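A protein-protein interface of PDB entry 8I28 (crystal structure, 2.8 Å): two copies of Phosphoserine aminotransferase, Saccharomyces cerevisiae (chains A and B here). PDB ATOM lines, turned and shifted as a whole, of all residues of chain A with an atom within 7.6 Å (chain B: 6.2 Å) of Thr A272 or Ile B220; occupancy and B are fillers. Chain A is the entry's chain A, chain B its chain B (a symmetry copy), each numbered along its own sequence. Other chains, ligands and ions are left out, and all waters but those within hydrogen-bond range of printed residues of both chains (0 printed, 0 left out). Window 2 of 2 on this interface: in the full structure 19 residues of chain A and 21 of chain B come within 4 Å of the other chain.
The backbone NH (N) of Gly B221 sits close to the backbone NH (N) of Thr A272.
N of Gly B78 is in hydrogen-bond range of O of Leu B222 (3.1 Å).
Among the printed residues, pairs that only touch across the chains: Leu A76 with Leu B222 (3.6 Å), Gln A77 with Leu B222 (3.7 Å), Ala A257 with Thr B81 (3.8 Å), Ala A257 with Leu B222 (3.8 Å), Thr A272 with Ile B220 (3.9 Å), Thr A272 with Leu B222 (3.7 Å) and Thr A272 with Ala B223 (3.3 Å).
Of the 11 printed residues of chain A, 4 touch a printed residue of chain B. Of the 14 printed residues of chain B, 5 touch a printed residue of chain A. Among the printed residues, no Asp or Glu carboxylate lies within 4 Å of a Lys or Arg side-chain nitrogen of the other chain.
Of chain B, only Ile B220 (3.9 Å), Gly B221 (2.9 Å), Leu B222 (3.7 Å) and Ala B223 (3.3 Å) come within 4 Å of Thr A272. Ile B220 touches just one residue of chain A: Thr A272. Of the printed residues of chain B, Ala A257 touches Thr B81 (3.8 Å) and Leu B222 (3.8 Å). Of the printed residues of chain B, Leu A76 touches Leu B222 (3.6 Å). Tyr A75 touches none of the printed residues of chain B. The nearest printed residue of chain A that does not touch Leu B222 is Pro A274 (4.8 Å).
No position is printed for both chains.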
ATOM      1  N   TYR A  75      14.382 -14.522   8.145  1.00  0.00           N
ATOM      2  CA  TYR A  75      15.388 -14.507   7.097  1.00  0.00           C
ATOM      3  C   TYR A  75      15.767 -13.072   6.777  1.00  0.00           C
ATOM      4  O   TYR A  75      14.985 -12.138   6.986  1.00  0.00           O
ATOM      5  CB  TYR A  75      14.900 -15.183   5.829  1.00  0.00           C
ATOM      6  CG  TYR A  75      14.168 -16.473   6.036  1.00  0.00           C
ATOM      7  CD1 TYR A  75      14.831 -17.686   5.961  1.00  0.00           C
ATOM      8  CD2 TYR A  75      12.799 -16.482   6.278  1.00  0.00           C
ATOM      9  CE1 TYR A  75      14.147 -18.890   6.126  1.00  0.00           C
ATOM     10  CE2 TYR A  75      12.103 -17.673   6.452  1.00  0.00           C
ATOM     11  CZ  TYR A  75      12.777 -18.875   6.370  1.00  0.00           C
ATOM     12  OH  TYR A  75      12.077 -20.052   6.544  1.00  0.00           O
ATOM     13  N   LEU A  76      16.986 -12.907   6.284  1.00  0.00           N
ATOM     14  CA  LEU A  76      17.471 -11.606   5.871  1.00  0.00           C
ATOM     15  C   LEU A  76      18.255 -11.788   4.589  1.00  0.00           C
ATOM     16  O   LEU A  76      18.856 -12.843   4.354  1.00  0.00           O
ATOM     17  CB  LEU A  76      18.352 -10.926   6.937  1.00  0.00           C
ATOM     18  CG  LEU A  76      17.681  -9.670   7.485  1.00  0.00           C
ATOM     19  CD1 LEU A  76      18.491  -9.023   8.609  1.00  0.00           C
ATOM     20  CD2 LEU A  76      17.434  -8.707   6.333  1.00  0.00           C
ATOM     21  N   GLN A  77      18.233 -10.757   3.758  1.00  0.00           N
ATOM     22  CA  GLN A  77      18.905 -10.822   2.477  1.00  0.00           C
ATOM     23  C   GLN A  77      20.371 -10.491   2.676  1.00  0.00           C
ATOM     24  O   GLN A  77      20.698  -9.463   3.275  1.00  0.00           O
ATOM     25  CB  GLN A  77      18.264  -9.859   1.481  1.00  0.00           C
ATOM     26  CG  GLN A  77      18.763 -10.055   0.059  1.00  0.00           C
ATOM     27  CD  GLN A  77      17.881 -10.992  -0.734  1.00  0.00           C
ATOM     28  OE1 GLN A  77      16.809 -11.391  -0.271  1.00  0.00           O
ATOM     29  NE2 GLN A  77      18.331 -11.363  -1.931  1.00  0.00           N
ATOM     30  N   ALA A 257      16.712  -1.312   8.648  1.00  0.00           N
ATOM     31  CA  ALA A 257      16.457  -2.430   7.740  1.00  0.00           C
ATOM     32  C   ALA A 257      17.010  -3.737   8.295  1.00  0.00           C
ATOM     33  O   ALA A 257      16.494  -4.809   7.963  1.00  0.00           O
ATOM     34  CB  ALA A 257      17.042  -2.156   6.349  1.00  0.00           C
ATOM     35  N   VAL A 263      12.711  -6.374  11.624  1.00  0.00           N
ATOM     36  CA  VAL A 263      12.736  -7.397  10.574  1.00  0.00           C
ATOM     37  C   VAL A 263      11.756  -8.519  10.876  1.00  0.00           C
ATOM     38  O   VAL A 263      11.187  -9.124   9.959  1.00  0.00           O
ATOM     39  CB  VAL A 263      14.155  -7.953  10.367  1.00  0.00           C
ATOM     40  CG1 VAL A 263      14.162  -8.899   9.195  1.00  0.00           C
ATOM     41  CG2 VAL A 263      15.139  -6.821  10.114  1.00  0.00           C
ATOM     42  N   ASN A 266       7.258  -7.362  10.690  1.00  0.00           N
ATOM     43  CA  ASN A 266       6.489  -7.814   9.541  1.00  0.00           C
ATOM     44  C   ASN A 266       7.381  -8.656   8.635  1.00  0.00           C
ATOM     45  O   ASN A 266       7.532  -9.861   8.863  1.00  0.00           O
ATOM     46  CB  ASN A 266       5.879  -6.617   8.805  1.00  0.00           C
ATOM     47  CG  ASN A 266       4.434  -6.330   9.240  1.00  0.00           C
ATOM     48  OD1 ASN A 266       3.715  -7.224   9.700  1.00  0.00           O
ATOM     49  ND2 ASN A 266       4.009  -5.075   9.095  1.00  0.00           N
ATOM     50  N   ASN A 267       8.004  -8.040   7.635  1.00  0.00           N
ATOM     51  CA  ASN A 267       8.808  -8.790   6.667  1.00  0.00           C
ATOM     52  C   ASN A 267      10.308  -8.700   6.965  1.00  0.00           C
ATOM     53  O   ASN A 267      11.081  -8.109   6.205  1.00  0.00           O
ATOM     54  CB  ASN A 267       8.521  -8.296   5.246  1.00  0.00           C
ATOM     55  CG  ASN A 267       7.031  -8.230   4.941  1.00  0.00           C
ATOM     56  OD1 ASN A 267       6.324  -9.235   5.017  1.00  0.00           O
ATOM     57  ND2 ASN A 267       6.550  -7.041   4.593  1.00  0.00           N
ATOM     58  N   THR A 272       9.848  -6.017   1.059  1.00  0.00           N
ATOM     59  CA  THR A 272       9.563  -7.261   1.761  1.00  0.00           C
ATOM     60  C   THR A 272      10.789  -8.181   1.727  1.00  0.00           C
ATOM     61  O   THR A 272      11.889  -7.758   2.096  1.00  0.00           O
ATOM     62  CB  THR A 272       8.320  -7.968   1.161  1.00  0.00           C
ATOM     63  OG1 THR A 272       8.196  -9.291   1.703  1.00  0.00           O
ATOM     64  CG2 THR A 272       8.388  -8.013  -0.375  1.00  0.00           C
ATOM     65  N   ILE A 273      10.611  -9.429   1.303  1.00  0.00           N
ATOM     66  CA  ILE A 273      11.704 -10.389   1.198  1.00  0.00           C
ATOM     67  C   ILE A 273      11.824 -10.813  -0.260  1.00  0.00           C
ATOM     68  O   ILE A 273      10.834 -11.239  -0.860  1.00  0.00           O
ATOM     69  CB  ILE A 273      11.497 -11.620   2.097  1.00  0.00           C
ATOM     70  CG1 ILE A 273      11.056 -11.191   3.506  1.00  0.00           C
ATOM     71  CG2 ILE A 273      12.788 -12.458   2.133  1.00  0.00           C
ATOM     72  CD1 ILE A 273       9.602 -11.527   3.850  1.00  0.00           C
ATOM     73  N   PRO A 274      13.012 -10.693  -0.884  1.00  0.00           N
ATOM     74  CA  PRO A 274      13.202 -11.260  -2.228  1.00  0.00           C
ATOM     75  C   PRO A 274      12.994 -12.767  -2.240  1.00  0.00           C
ATOM     76  O   PRO A 274      13.833 -13.528  -1.742  1.00  0.00           O
ATOM     77  CB  PRO A 274      14.646 -10.874  -2.567  1.00  0.00           C
ATOM     78  CG  PRO A 274      14.833  -9.593  -1.835  1.00  0.00           C
ATOM     79  CD  PRO A 274      14.119  -9.796  -0.515  1.00  0.00           C
ATOM     80  N   ILE A 275      11.874 -13.192  -2.831  1.00  0.00           N
ATOM     81  CA  ILE A 275      11.356 -14.551  -2.708  1.00  0.00           C
ATOM     82  C   ILE A 275      11.737 -15.401  -3.915  1.00  0.00           C
ATOM     83  O   ILE A 275      12.914 -15.455  -4.294  1.00  0.00           O
ATOM     84  CB  ILE A 275       9.829 -14.525  -2.495  1.00  0.00           C
ATOM     85  CG1 ILE A 275       9.141 -13.582  -3.494  1.00  0.00           C
ATOM     86  CG2 ILE A 275       9.511 -14.100  -1.064  1.00  0.00           C
ATOM     87  CD1 ILE A 275       7.660 -13.346  -3.215  1.00  0.00           C
ATOM     88  N   GLY B  78      17.803  -2.623  -1.856  1.00  0.00           N
ATOM     89  CA  GLY B  78      17.281  -1.836  -0.761  1.00  0.00           C
ATOM     90  C   GLY B  78      16.005  -1.082  -1.047  1.00  0.00           C
ATOM     91  O   GLY B  78      15.042  -1.198  -0.286  1.00  0.00           O
ATOM     92  N   GLY B  79      15.991  -0.267  -2.095  1.00  0.00           N
ATOM     93  CA  GLY B  79      14.774   0.419  -2.493  1.00  0.00           C
ATOM     94  C   GLY B  79      14.006   1.220  -1.450  1.00  0.00           C
ATOM     95  O   GLY B  79      12.908   1.702  -1.739  1.00  0.00           O
ATOM     96  N   GLY B  80      14.538   1.378  -0.240  1.00  0.00           N
ATOM     97  CA  GLY B  80      13.809   2.159   0.738  1.00  0.00           C
ATOM     98  C   GLY B  80      14.655   2.742   1.848  1.00  0.00           C
ATOM     99  O   GLY B  80      15.488   3.627   1.625  1.00  0.00           O
ATOM    100  N   THR B  81      14.400   2.238   3.060  1.00  0.00           N
ATOM    101  CA  THR B  81      15.150   2.591   4.261  1.00  0.00           C
ATOM    102  C   THR B  81      16.650   2.488   4.031  1.00  0.00           C
ATOM    103  O   THR B  81      17.405   3.411   4.352  1.00  0.00           O
ATOM    104  CB  THR B  81      14.714   1.667   5.398  1.00  0.00           C
ATOM    105  OG1 THR B  81      13.426   2.077   5.869  1.00  0.00           O
ATOM    106  CG2 THR B  81      15.718   1.671   6.548  1.00  0.00           C
ATOM    107  N   TRP B 113       9.058  11.409   3.659  1.00  0.00           N
ATOM    108  CA  TRP B 113      10.308  10.722   3.348  1.00  0.00           C
ATOM    109  C   TRP B 113      11.510  11.523   3.832  1.00  0.00           C
ATOM    110  O   TRP B 113      12.413  10.969   4.468  1.00  0.00           O
ATOM    111  CB  TRP B 113      10.418  10.441   1.846  1.00  0.00           C
ATOM    112  CG  TRP B 113      11.280   9.263   1.573  1.00  0.00           C
ATOM    113  CD1 TRP B 113      12.460   9.258   0.882  1.00  0.00           C
ATOM    114  CD2 TRP B 113      11.024   7.897   1.949  1.00  0.00           C
ATOM    115  NE1 TRP B 113      12.971   7.974   0.829  1.00  0.00           N
ATOM    116  CE2 TRP B 113      12.106   7.119   1.468  1.00  0.00           C
ATOM    117  CE3 TRP B 113       9.994   7.256   2.653  1.00  0.00           C
ATOM    118  CZ2 TRP B 113      12.188   5.740   1.671  1.00  0.00           C
ATOM    119  CZ3 TRP B 113      10.081   5.878   2.852  1.00  0.00           C
ATOM    120  CH2 TRP B 113      11.171   5.140   2.365  1.00  0.00           C
ATOM    121  N   ALA B 216      12.254   3.228  -4.387  1.00  0.00           N
ATOM    122  CA  ALA B 216      10.895   3.610  -4.058  1.00  0.00           C
ATOM    123  C   ALA B 216      10.909   4.673  -2.954  1.00  0.00           C
ATOM    124  O   ALA B 216      11.956   5.141  -2.493  1.00  0.00           O
ATOM    125  CB  ALA B 216      10.086   2.385  -3.633  1.00  0.00           C
ATOM    126  N   LYS B 218       8.908   3.734  -0.271  1.00  0.00           N
ATOM    127  CA  LYS B 218       8.133   2.834   0.572  1.00  0.00           C
ATOM    128  C   LYS B 218       9.053   2.172   1.585  1.00  0.00           C
ATOM    129  O   LYS B 218      10.195   1.820   1.271  1.00  0.00           O
ATOM    130  CB  LYS B 218       7.390   1.759  -0.260  1.00  0.00           C
ATOM    131  CG  LYS B 218       6.202   2.303  -1.077  1.00  0.00           C
ATOM    132  CD  LYS B 218       6.610   2.704  -2.504  1.00  0.00           C
ATOM    133  CE  LYS B 218       5.682   3.759  -3.126  1.00  0.00           C
ATOM    134  NZ  LYS B 218       5.572   5.044  -2.335  1.00  0.00           N
ATOM    135  N   ASN B 219       8.559   2.028   2.811  1.00  0.00           N
ATOM    136  CA  ASN B 219       9.300   1.277   3.814  1.00  0.00           C
ATOM    137  C   ASN B 219       9.216  -0.207   3.485  1.00  0.00           C
ATOM    138  O   ASN B 219       8.750  -1.001   4.306  1.00  0.00           O
ATOM    139  CB  ASN B 219       8.773   1.535   5.239  1.00  0.00           C
ATOM    140  CG  ASN B 219       8.280   2.972   5.459  1.00  0.00           C
ATOM    141  OD1 ASN B 219       7.202   3.361   4.995  1.00  0.00           O
ATOM    142  ND2 ASN B 219       9.067   3.756   6.190  1.00  0.00           N
ATOM    143  N   ILE B 220       9.646  -0.589   2.282  1.00  0.00           N
ATOM    144  CA  ILE B 220       9.735  -1.997   1.917  1.00  0.00           C
ATOM    145  C   ILE B 220      10.956  -2.551   2.640  1.00  0.00           C
ATOM    146  O   ILE B 220      11.624  -1.825   3.391  1.00  0.00           O
ATOM    147  CB  ILE B 220       9.824  -2.200   0.393  1.00  0.00           C
ATOM    148  CG1 ILE B 220      10.924  -1.337  -0.211  1.00  0.00           C
ATOM    149  CG2 ILE B 220       8.518  -1.798  -0.266  1.00  0.00           C
ATOM    150  CD1 ILE B 220      10.842  -1.230  -1.726  1.00  0.00           C
ATOM    151  N   GLY B 221      11.253  -3.831   2.440  1.00  0.00           N
ATOM    152  CA  GLY B 221      12.327  -4.448   3.195  1.00  0.00           C
ATOM    153  C   GLY B 221      13.694  -4.096   2.656  1.00  0.00           C
ATOM    154  O   GLY B 221      14.031  -2.919   2.497  1.00  0.00           O
ATOM    155  N   LEU B 222      14.507  -5.115   2.407  1.00  0.00           N
ATOM    156  CA  LEU B 222      15.654  -4.988   1.523  1.00  0.00           C
ATOM    157  C   LEU B 222      15.258  -5.189   0.068  1.00  0.00           C
ATOM    158  O   LEU B 222      16.105  -5.053  -0.826  1.00  0.00           O
ATOM    159  CB  LEU B 222      16.735  -5.989   1.922  1.00  0.00           C
ATOM    160  CG  LEU B 222      17.726  -5.467   2.953  1.00  0.00           C
ATOM    161  CD1 LEU B 222      17.181  -5.670   4.355  1.00  0.00           C
ATOM    162  CD2 LEU B 222      19.010  -6.237   2.736  1.00  0.00           C
ATOM    163  N   ALA B 223      13.980  -5.477  -0.173  1.00  0.00           N
ATOM    164  CA  ALA B 223      13.466  -5.720  -1.509  1.00  0.00           C
ATOM    165  C   ALA B 223      13.584  -4.474  -2.384  1.00  0.00           C
ATOM    166  O   ALA B 223      13.685  -3.339  -1.910  1.00  0.00           O
ATOM    167  CB  ALA B 223      12.011  -6.178  -1.429  1.00  0.00           C
ATOM    168  N   GLY B 224      13.564  -4.699  -3.684  1.00  0.00           N
ATOM    169  CA  GLY B 224      13.709  -3.615  -4.618  1.00  0.00           C
ATOM    170  C   GLY B 224      15.153  -3.204  -4.757  1.00  0.00           C
ATOM    171  O   GLY B 224      16.085  -3.810  -4.222  1.00  0.00           O
ATOM    172  N   LEU B 225      15.331  -2.130  -5.502  1.00  0.00           N
ATOM    173  CA  LEU B 225      16.648  -1.613  -5.807  1.00  0.00           C
ATOM    174  C   LEU B 225      16.606  -0.098  -5.663  1.00  0.00           C
ATOM    175  O   LEU B 225      15.576   0.533  -5.935  1.00  0.00           O
ATOM    176  CB  LEU B 225      17.058  -2.036  -7.218  1.00  0.00           C
ATOM    177  CG  LEU B 225      18.486  -1.823  -7.686  1.00  0.00           C
ATOM    178  CD1 LEU B 225      19.253  -3.142  -7.656  1.00  0.00           C
ATOM    179  CD2 LEU B 225      18.457  -1.232  -9.080  1.00  0.00           C
